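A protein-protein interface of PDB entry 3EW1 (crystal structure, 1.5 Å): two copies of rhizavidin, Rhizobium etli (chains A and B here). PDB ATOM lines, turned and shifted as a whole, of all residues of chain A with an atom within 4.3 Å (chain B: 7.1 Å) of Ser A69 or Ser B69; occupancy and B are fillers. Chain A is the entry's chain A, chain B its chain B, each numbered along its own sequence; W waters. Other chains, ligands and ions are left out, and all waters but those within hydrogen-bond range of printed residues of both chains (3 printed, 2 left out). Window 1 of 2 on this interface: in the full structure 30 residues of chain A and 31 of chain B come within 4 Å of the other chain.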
ATOM      1  N   PRO A  56     -16.625  15.099  32.040  1.00  0.00           N
ATOM      2  CA  PRO A  56     -17.850  15.404  32.777  1.00  0.00           C
ATOM      3  C   PRO A  56     -19.084  14.770  32.184  1.00  0.00           C
ATOM      4  O   PRO A  56     -19.243  14.692  30.941  1.00  0.00           O
ATOM      5  CB  PRO A  56     -17.954  16.946  32.696  1.00  0.00           C
ATOM      6  CG  PRO A  56     -16.481  17.384  32.399  1.00  0.00           C
ATOM      7  CD  PRO A  56     -15.969  16.321  31.519  1.00  0.00           C
ATOM      8  N   LEU A  57     -19.977  14.315  33.062  1.00  0.00           N
ATOM      9  CA  LEU A  57     -21.232  13.707  32.649  1.00  0.00           C
ATOM     10  C   LEU A  57     -22.375  14.372  33.422  1.00  0.00           C
ATOM     11  O   LEU A  57     -22.266  14.597  34.631  1.00  0.00           O
ATOM     12  CB  LEU A  57     -21.215  12.169  32.847  1.00  0.00           C
ATOM     13  CG  LEU A  57     -21.650  11.413  34.099  1.00  0.00           C
ATOM     14  CD1 LEU A  57     -23.118  11.641  34.465  1.00  0.00           C
ATOM     15  CD2 LEU A  57     -21.390   9.972  33.828  1.00  0.00           C
ATOM     16  N   THR A  58     -23.462  14.706  32.738  1.00  0.00           N
ATOM     17  CA  THR A  58     -24.629  15.265  33.422  1.00  0.00           C
ATOM     18  C   THR A  58     -25.844  14.408  33.018  1.00  0.00           C
ATOM     19  O   THR A  58     -25.771  13.628  32.051  1.00  0.00           O
ATOM     20  CB  THR A  58     -24.835  16.747  33.064  1.00  0.00           C
ATOM     21  OG1 THR A  58     -25.746  17.392  33.968  1.00  0.00           O
ATOM     22  CG2 THR A  58     -25.367  16.827  31.675  1.00  0.00           C
ATOM     23  N   GLY A  59     -26.943  14.518  33.767  1.00  0.00           N
ATOM     24  CA  GLY A  59     -28.178  13.878  33.355  1.00  0.00           C
ATOM     25  C   GLY A  59     -29.324  14.119  34.297  1.00  0.00           C
ATOM     26  O   GLY A  59     -29.249  15.012  35.173  1.00  0.00           O
ATOM     27  N   ARG A  60     -30.364  13.311  34.120  1.00  0.00           N
ATOM     28  CA  ARG A  60     -31.605  13.461  34.858  1.00  0.00           C
ATOM     29  C   ARG A  60     -32.158  12.072  35.146  1.00  0.00           C
ATOM     30  O   ARG A  60     -31.997  11.141  34.339  1.00  0.00           O
ATOM     31  CB  ARG A  60     -32.677  14.254  34.085  1.00  0.00           C
ATOM     32  CG  ARG A  60     -32.361  15.775  33.900  1.00  0.00           C
ATOM     33  CD  ARG A  60     -32.428  16.501  35.269  1.00  0.00           C
ATOM     34  NE  ARG A  60     -33.788  16.412  35.802  1.00  0.00           N
ATOM     35  CZ  ARG A  60     -34.173  16.830  37.004  1.00  0.00           C
ATOM     36  NH1 ARG A  60     -33.303  17.387  37.827  1.00  0.00           N
ATOM     37  NH2 ARG A  60     -35.444  16.680  37.384  1.00  0.00           N
ATOM     38  N   ALA A  67     -31.392   9.396  31.968  1.00  0.00           N
ATOM     39  CA  ALA A  67     -30.710   9.824  30.736  1.00  0.00           C
ATOM     40  C   ALA A  67     -29.486  10.654  31.123  1.00  0.00           C
ATOM     41  O   ALA A  67     -29.555  11.517  31.978  1.00  0.00           O
ATOM     42  CB  ALA A  67     -31.628  10.620  29.854  1.00  0.00           C
ATOM     43  N   PHE A  68     -28.368  10.425  30.436  1.00  0.00           N
ATOM     44  CA  PHE A  68     -27.165  11.181  30.773  1.00  0.00           C
ATOM     45  C   PHE A  68     -26.322  11.486  29.547  1.00  0.00           C
ATOM     46  O   PHE A  68     -26.500  10.827  28.523  1.00  0.00           O
ATOM     47  CB  PHE A  68     -26.389  10.544  31.931  1.00  0.00           C
ATOM     48  CG  PHE A  68     -25.874   9.178  31.641  1.00  0.00           C
ATOM     49  CD1 PHE A  68     -26.620   8.034  31.967  1.00  0.00           C
ATOM     50  CD2 PHE A  68     -24.591   9.015  31.132  1.00  0.00           C
ATOM     51  CE1 PHE A  68     -26.118   6.797  31.708  1.00  0.00           C
ATOM     52  CE2 PHE A  68     -24.071   7.743  30.926  1.00  0.00           C
ATOM     53  CZ  PHE A  68     -24.858   6.637  31.199  1.00  0.00           C
ATOM     54  N   SER A  69     -25.414  12.439  29.677  1.00  0.00           N
ATOM     55  CA  SER A  69     -24.812  13.044  28.455  1.00  0.00           C
ATOM     56  C   SER A  69     -23.331  13.279  28.772  1.00  0.00           C
ATOM     57  O   SER A  69     -22.979  13.667  29.903  1.00  0.00           O
ATOM     58  CB  SER A  69     -25.461  14.395  28.133  1.00  0.00           C
ATOM     59  OG  SER A  69     -26.883  14.294  27.890  1.00  0.00           O
ATOM     60  N   VAL A  70     -22.477  13.075  27.775  1.00  0.00           N
ATOM     61  CA  VAL A  70     -21.035  13.344  27.884  1.00  0.00           C
ATOM     62  C   VAL A  70     -20.636  14.044  26.580  1.00  0.00           C
ATOM     63  O   VAL A  70     -20.972  13.604  25.460  1.00  0.00           O
ATOM     64  CB  VAL A  70     -20.185  12.042  28.115  1.00  0.00           C
ATOM     65  CG1 VAL A  70     -18.683  12.328  28.051  1.00  0.00           C
ATOM     66  CG2 VAL A  70     -20.504  11.419  29.469  1.00  0.00           C
ATOM     67  N   THR A  83     -21.985  11.988  23.320  1.00  0.00           N
ATOM     68  CA  THR A  83     -22.842  10.823  23.515  1.00  0.00           C
ATOM     69  C   THR A  83     -23.964  11.043  24.532  1.00  0.00           C
ATOM     70  O   THR A  83     -23.733  11.668  25.570  1.00  0.00           O
ATOM     71  CB  THR A  83     -21.973   9.634  24.008  1.00  0.00           C
ATOM     72  OG1 THR A  83     -20.893   9.424  23.082  1.00  0.00           O
ATOM     73  CG2 THR A  83     -22.777   8.347  24.155  1.00  0.00           C
ATOM     74  N   GLY B  39     -31.208  23.932  31.468  1.00  0.00           N
ATOM     75  CA  GLY B  39     -32.354  24.566  30.876  1.00  0.00           C
ATOM     76  C   GLY B  39     -33.641  23.949  31.284  1.00  0.00           C
ATOM     77  O   GLY B  39     -33.686  23.214  32.260  1.00  0.00           O
ATOM     78  N   TYR B  41     -37.406  22.296  29.543  1.00  0.00           N
ATOM     79  CA  TYR B  41     -38.037  21.806  28.344  1.00  0.00           C
ATOM     80  C   TYR B  41     -39.553  21.783  28.557  1.00  0.00           C
ATOM     81  O   TYR B  41     -40.050  21.375  29.631  1.00  0.00           O
ATOM     82  CB  TYR B  41     -37.502  20.396  28.067  1.00  0.00           C
ATOM     83  CG  TYR B  41     -37.900  19.800  26.735  1.00  0.00           C
ATOM     84  CD1 TYR B  41     -39.163  19.250  26.534  1.00  0.00           C
ATOM     85  CD2 TYR B  41     -36.979  19.759  25.674  1.00  0.00           C
ATOM     86  CE1 TYR B  41     -39.513  18.695  25.266  1.00  0.00           C
ATOM     87  CE2 TYR B  41     -37.301  19.191  24.464  1.00  0.00           C
ATOM     88  CZ  TYR B  41     -38.564  18.669  24.266  1.00  0.00           C
ATOM     89  OH  TYR B  41     -38.865  18.123  23.042  1.00  0.00           O
ATOM     90  N   TYR B  55     -39.844  21.119  32.409  1.00  0.00           N
ATOM     91  CA  TYR B  55     -39.053  20.009  32.964  1.00  0.00           C
ATOM     92  C   TYR B  55     -37.574  20.359  32.877  1.00  0.00           C
ATOM     93  O   TYR B  55     -37.116  20.829  31.844  1.00  0.00           O
ATOM     94  CB  TYR B  55     -39.333  18.751  32.171  1.00  0.00           C
ATOM     95  CG  TYR B  55     -40.674  18.199  32.534  1.00  0.00           C
ATOM     96  CD1 TYR B  55     -41.816  18.634  31.870  1.00  0.00           C
ATOM     97  CD2 TYR B  55     -40.827  17.268  33.587  1.00  0.00           C
ATOM     98  CE1 TYR B  55     -43.093  18.169  32.216  1.00  0.00           C
ATOM     99  CE2 TYR B  55     -42.098  16.770  33.894  1.00  0.00           C
ATOM    100  CZ  TYR B  55     -43.227  17.243  33.213  1.00  0.00           C
ATOM    101  OH  TYR B  55     -44.517  16.845  33.472  1.00  0.00           O
ATOM    102  N   PRO B  56     -36.812  20.121  33.951  1.00  0.00           N
ATOM    103  CA  PRO B  56     -35.371  20.420  33.916  1.00  0.00           C
ATOM    104  C   PRO B  56     -34.672  19.632  32.822  1.00  0.00           C
ATOM    105  O   PRO B  56     -34.990  18.471  32.524  1.00  0.00           O
ATOM    106  CB  PRO B  56     -34.886  19.933  35.305  1.00  0.00           C
ATOM    107  CG  PRO B  56     -36.135  20.087  36.188  1.00  0.00           C
ATOM    108  CD  PRO B  56     -37.241  19.604  35.270  1.00  0.00           C
ATOM    109  N   LEU B  57     -33.709  20.296  32.202  1.00  0.00           N
ATOM    110  CA  LEU B  57     -32.852  19.656  31.242  1.00  0.00           C
ATOM    111  C   LEU B  57     -31.417  19.934  31.582  1.00  0.00           C
ATOM    112  O   LEU B  57     -31.070  20.989  32.120  1.00  0.00           O
ATOM    113  CB  LEU B  57     -33.236  20.175  29.858  1.00  0.00           C
ATOM    114  CG  LEU B  57     -32.591  20.875  28.685  1.00  0.00           C
ATOM    115  CD1 LEU B  57     -31.062  20.989  28.493  1.00  0.00           C
ATOM    116  CD2 LEU B  57     -33.325  20.454  27.409  1.00  0.00           C
ATOM    117  N   THR B  58     -30.573  18.963  31.288  1.00  0.00           N
ATOM    118  CA  THR B  58     -29.141  19.116  31.536  1.00  0.00           C
ATOM    119  C   THR B  58     -28.387  18.442  30.403  1.00  0.00           C
ATOM    120  O   THR B  58     -28.892  17.531  29.790  1.00  0.00           O
ATOM    121  CB  THR B  58     -28.792  18.515  32.893  1.00  0.00           C
ATOM    122  OG1 THR B  58     -27.449  18.849  33.245  1.00  0.00           O
ATOM    123  CG2 THR B  58     -29.014  17.057  32.836  1.00  0.00           C
ATOM    124  N   GLY B  59     -27.168  18.862  30.119  1.00  0.00           N
ATOM    125  CA  GLY B  59     -26.489  18.375  28.914  1.00  0.00           C
ATOM    126  C   GLY B  59     -25.031  18.806  28.881  1.00  0.00           C
ATOM    127  O   GLY B  59     -24.545  19.488  29.821  1.00  0.00           O
ATOM    128  N   ARG B  60     -24.350  18.468  27.778  1.00  0.00           N
ATOM    129  CA  ARG B  60     -22.948  18.834  27.561  1.00  0.00           C
ATOM    130  C   ARG B  60     -22.764  19.192  26.109  1.00  0.00           C
ATOM    131  O   ARG B  60     -23.438  18.639  25.263  1.00  0.00           O
ATOM    132  CB  ARG B  60     -21.989  17.677  27.891  1.00  0.00           C
ATOM    133  CG  ARG B  60     -21.930  17.267  29.416  1.00  0.00           C
ATOM    134  CD  ARG B  60     -21.119  18.239  30.300  1.00  0.00           C
ATOM    135  NE  ARG B  60     -19.770  18.455  29.756  1.00  0.00           N
ATOM    136  CZ  ARG B  60     -18.925  19.449  30.052  1.00  0.00           C
ATOM    137  NH1 ARG B  60     -19.225  20.376  30.960  1.00  0.00           N
ATOM    138  NH2 ARG B  60     -17.759  19.516  29.397  1.00  0.00           N
ATOM    139  N   ILE B  66     -23.782  18.190  20.765  1.00  0.00           N
ATOM    140  CA  ILE B  66     -24.498  18.401  22.009  1.00  0.00           C
ATOM    141  C   ILE B  66     -25.256  17.157  22.360  1.00  0.00           C
ATOM    142  O   ILE B  66     -25.786  16.436  21.515  1.00  0.00           O
ATOM    143  CB  ILE B  66     -25.485  19.625  21.913  1.00  0.00           C
ATOM    144  CG1 ILE B  66     -26.139  19.907  23.279  1.00  0.00           C
ATOM    145  CG2 ILE B  66     -26.522  19.433  20.797  1.00  0.00           C
ATOM    146  CD1 ILE B  66     -26.979  21.206  23.332  1.00  0.00           C
ATOM    147  N   ALA B  67     -25.314  16.907  23.658  1.00  0.00           N
ATOM    148  CA  ALA B  67     -26.183  15.832  24.185  1.00  0.00           C
ATOM    149  C   ALA B  67     -26.903  16.397  25.395  1.00  0.00           C
ATOM    150  O   ALA B  67     -26.289  17.058  26.245  1.00  0.00           O
ATOM    151  CB  ALA B  67     -25.373  14.576  24.522  1.00  0.00           C
ATOM    152  N   PHE B  68     -28.208  16.129  25.511  1.00  0.00           N
ATOM    153  CA  PHE B  68     -28.939  16.650  26.649  1.00  0.00           C
ATOM    154  C   PHE B  68     -30.025  15.670  27.067  1.00  0.00           C
ATOM    155  O   PHE B  68     -30.413  14.763  26.311  1.00  0.00           O
ATOM    156  CB  PHE B  68     -29.465  18.078  26.401  1.00  0.00           C
ATOM    157  CG  PHE B  68     -30.371  18.229  25.209  1.00  0.00           C
ATOM    158  CD1 PHE B  68     -29.840  18.469  23.936  1.00  0.00           C
ATOM    159  CD2 PHE B  68     -31.745  18.155  25.352  1.00  0.00           C
ATOM    160  CE1 PHE B  68     -30.677  18.643  22.834  1.00  0.00           C
ATOM    161  CE2 PHE B  68     -32.605  18.349  24.248  1.00  0.00           C
ATOM    162  CZ  PHE B  68     -32.056  18.568  22.998  1.00  0.00           C
ATOM    163  N   SER B  69     -30.544  15.881  28.268  1.00  0.00           N
ATOM    164  CA  SER B  69     -31.346  14.846  28.988  1.00  0.00           C
ATOM    165  C   SER B  69     -32.492  15.474  29.776  1.00  0.00           C
ATOM    166  O   SER B  69     -32.306  16.545  30.384  1.00  0.00           O
ATOM    167  CB  SER B  69     -30.442  14.124  29.996  1.00  0.00           C
ATOM    168  OG  SER B  69     -29.344  13.464  29.384  1.00  0.00           O
ATOM    169  N   VAL B  70     -33.656  14.804  29.791  1.00  0.00           N
ATOM    170  CA  VAL B  70     -34.825  15.284  30.531  1.00  0.00           C
ATOM    171  C   VAL B  70     -35.430  14.064  31.212  1.00  0.00           C
ATOM    172  O   VAL B  70     -35.644  13.045  30.569  1.00  0.00           O
ATOM    173  CB  VAL B  70     -35.873  15.968  29.578  1.00  0.00           C
ATOM    174  CG1 VAL B  70     -37.167  16.277  30.279  1.00  0.00           C
ATOM    175  CG2 VAL B  70     -35.292  17.270  28.938  1.00  0.00           C
ATOM    176  N   GLY B  71     -35.637  14.151  32.535  1.00  0.00           N
ATOM    177  CA  GLY B  71     -36.472  13.178  33.270  1.00  0.00           C
ATOM    178  C   GLY B  71     -37.895  13.734  33.336  1.00  0.00           C
ATOM    179  O   GLY B  71     -38.083  14.954  33.485  1.00  0.00           O
ATOM    180  N   ALA B  82     -37.729   8.942  30.716  1.00  0.00           N
ATOM    181  CA  ALA B  82     -36.578   9.849  30.528  1.00  0.00           C
ATOM    182  C   ALA B  82     -36.235   9.860  29.076  1.00  0.00           C
ATOM    183  O   ALA B  82     -36.333   8.829  28.444  1.00  0.00           O
ATOM    184  CB  ALA B  82     -35.369   9.388  31.330  1.00  0.00           C
ATOM    185  N   THR B  83     -35.774  11.007  28.561  1.00  0.00           N
ATOM    186  CA  THR B  83     -35.380  11.120  27.161  1.00  0.00           C
ATOM    187  C   THR B  83     -33.986  11.694  27.090  1.00  0.00           C
ATOM    188  O   THR B  83     -33.607  12.603  27.864  1.00  0.00           O
ATOM    189  CB  THR B  83     -36.343  12.047  26.460  1.00  0.00           C
ATOM    190  OG1 THR B  83     -37.667  11.526  26.477  1.00  0.00           O
ATOM    191  CG2 THR B  83     -35.965  12.220  25.017  1.00  0.00           C
ATOM    192  N   GLY B  84     -33.227  11.173  26.131  1.00  0.00           N
ATOM    193  CA  GLY B  84     -31.882  11.631  25.900  1.00  0.00           C
ATOM    194  C   GLY B  84     -31.827  12.032  24.444  1.00  0.00           C
ATOM    195  O   GLY B  84     -32.191  11.225  23.594  1.00  0.00           O
ATOM    196  N   TRP B  85     -31.329  13.230  24.154  1.00  0.00           N
ATOM    197  CA  TRP B  85     -31.102  13.675  22.781  1.00  0.00           C
ATOM    198  C   TRP B  85     -29.616  13.810  22.535  1.00  0.00           C
ATOM    199  O   TRP B  85     -28.849  14.262  23.404  1.00  0.00           O
ATOM    200  CB  TRP B  85     -31.729  15.039  22.529  1.00  0.00           C
ATOM    201  CG  TRP B  85     -33.224  15.209  22.603  1.00  0.00           C
ATOM    202  CD1 TRP B  85     -34.073  15.406  21.531  1.00  0.00           C
ATOM    203  CD2 TRP B  85     -34.025  15.360  23.772  1.00  0.00           C
ATOM    204  NE1 TRP B  85     -35.350  15.645  21.973  1.00  0.00           N
ATOM    205  CE2 TRP B  85     -35.358  15.576  23.345  1.00  0.00           C
ATOM    206  CE3 TRP B  85     -33.747  15.300  25.147  1.00  0.00           C
ATOM    207  CZ2 TRP B  85     -36.414  15.770  24.231  1.00  0.00           C
ATOM    208  CZ3 TRP B  85     -34.808  15.464  26.027  1.00  0.00           C
ATOM    209  CH2 TRP B  85     -36.123  15.714  25.569  1.00  0.00           C
ATOM    210  N   THR B  86     -29.208  13.471  21.319  1.00  0.00           N
ATOM    211  CA  THR B  86     -27.808  13.639  20.910  1.00  0.00           C
ATOM    212  C   THR B  86     -27.839  14.192  19.490  1.00  0.00           C
ATOM    213  O   THR B  86     -28.641  13.725  18.701  1.00  0.00           O
ATOM    214  CB  THR B  86     -27.075  12.260  20.972  1.00  0.00           C
ATOM    215  OG1 THR B  86     -27.407  11.576  22.197  1.00  0.00           O
ATOM    216  CG2 THR B  86     -25.573  12.452  20.886  1.00  0.00           C
HETATM  217  O   HOH W   1     -37.189  14.132  36.391  1.00  0.00           O
HETATM  218  O   HOH W   2     -18.383  16.097  28.979  1.00  0.00           O
HETATM  219  O   HOH W   3     -36.002  16.554  34.119  1.00  0.00           O
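The side-chain hydroxyl (OG) of Ser B69 sits at hydrogen-bond distance from the backbone carbonyl oxygen (O) of Ala A67 (3.3 Å).
The side-chain hydroxyl (OG) of Ser B69 sits at hydrogen-bond distance from the backbone NH (N) of Phe A68 (3.4 Å).
O of Ala B67 lies close to OG of Ser A69, at 3.3 Å.
OG of Ser A69 lies within hydrogen-bond range of N of Phe B68, 3.3 Å away.
The side-chain hydroxyl (OG) of Ser A69 lies within hydrogen-bond range of the side-chain hydroxyl (OG) of Ser B69 (3.0 Å).
OG1 of Thr A58 lies close to OG1 of Thr B58, 2.4 Å away.
The backbone carbonyl oxygen (O) of Thr A58 is in hydrogen-bond range of the backbone NH (N) of Ser A69.
The backbone carbonyl oxygen (O) of Ala A67 sits at hydrogen-bond distance from the backbone NH (N) of Arg A60 (2.9 Å).
O of Val A70 sits at hydrogen-bond distance from N of Thr A83 (2.9 Å).
The backbone carbonyl oxygen of Ala B67 lies within hydrogen-bond range of the backbone NH of Arg B60 (2.8 Å).
N of Trp B85 is in hydrogen-bond range of O of Phe B68 (2.8 Å).
The backbone NH of Thr B83 sits at hydrogen-bond distance from the backbone carbonyl oxygen of Val B70 (2.9 Å).
Among the printed residues, pairs that only touch across the chains: Pro A56 with Arg B60 (3.8 Å), Thr A58 with Gly B59 (3.1 Å), Gly A59 with Thr B58 (3.1 Å), Arg A60 with Pro B56 (3.6 Å), Arg A60 with Thr B58 (3.7 Å), Arg A60 with Ser B69 (3.6 Å), Arg A60 with Val B70 (3.98 Å), Arg A60 with Gly B71 (3.3 Å), Ala A67 with Thr B83 (3.4 Å), Ser A69 with Arg B60 (3.8 Å) and Thr A83 with Ala B67 (3.5 Å).
Of the printed residues of chain B, Gly A59 touches Thr B58.
Ser A69 touches just these residues of chain B: Arg B60, Ala B67, Phe B68 and Ser B69.
Printed residues of chain A within 4 Å of Arg B60: Pro A56 (3.8 Å) and Ser A69 (3.8 Å).
Of chain A, only Arg A60, Ala A67, Phe A68 and Ser A69 come within 4 Å of Ser B69.
The nearest residue of chain B that does not touch Ser A69 is Gly B59 (4.2 Å).
The nearest printed residue of chain B that does not touch Pro A56 is Gly B59 (7.2 Å).
Of the 10 printed residues of chain A, 8 touch a printed residue of chain B.
Hydrophobic or aromatic side chains of chain A within 4 Å of the printed part of chain B: Pro A56 and Ala A67.
Along chain A the printed residues that touch a printed residue of chain B span positions 56 to 83.
Of the 19 printed residues of chain B, 10 touch a printed residue of chain A.
Printed residues of chain B that touch a printed residue of chain A: Pro B56, Thr B58, Gly B59, Arg B60, Ala B67, Phe B68, Ser B69, Val B70, Gly B71 and Thr B83.
Among the printed residues, 17 pairs touch across the chains.
Thr A58 touches Gly B59, and with the chains exchanged Gly A59 touches Thr B58.
Arg A60 touches Ser B69, and with the chains exchanged Ser A69 touches Arg B60.
Ala A67 touches Thr B83, and with the chains exchanged Thr A83 touches Ala B67.
Phe A68 touches Ser B69, and with the chains exchanged Ser A69 touches Phe B68.
10 positions are printed for both chains.
Water W2 lies within hydrogen-bond range of the backbone carbonyl oxygen of Pro A56 (2.6 Å) and the guanidinium group of Arg B60 (2.8 Å).
Water W3 lies within hydrogen-bond range of the backbone carbonyl oxygen of Pro B56 (2.7 Å), the backbone carbonyl oxygen of Gly B71 (2.7 Å) and the guanidinium group of Arg A60 (2.8 Å).
Water W1 bridges the backbone carbonyl oxygen of Gly B71 (3.1 Å) and the guanidinium group of Arg A60 (3.2 Å).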
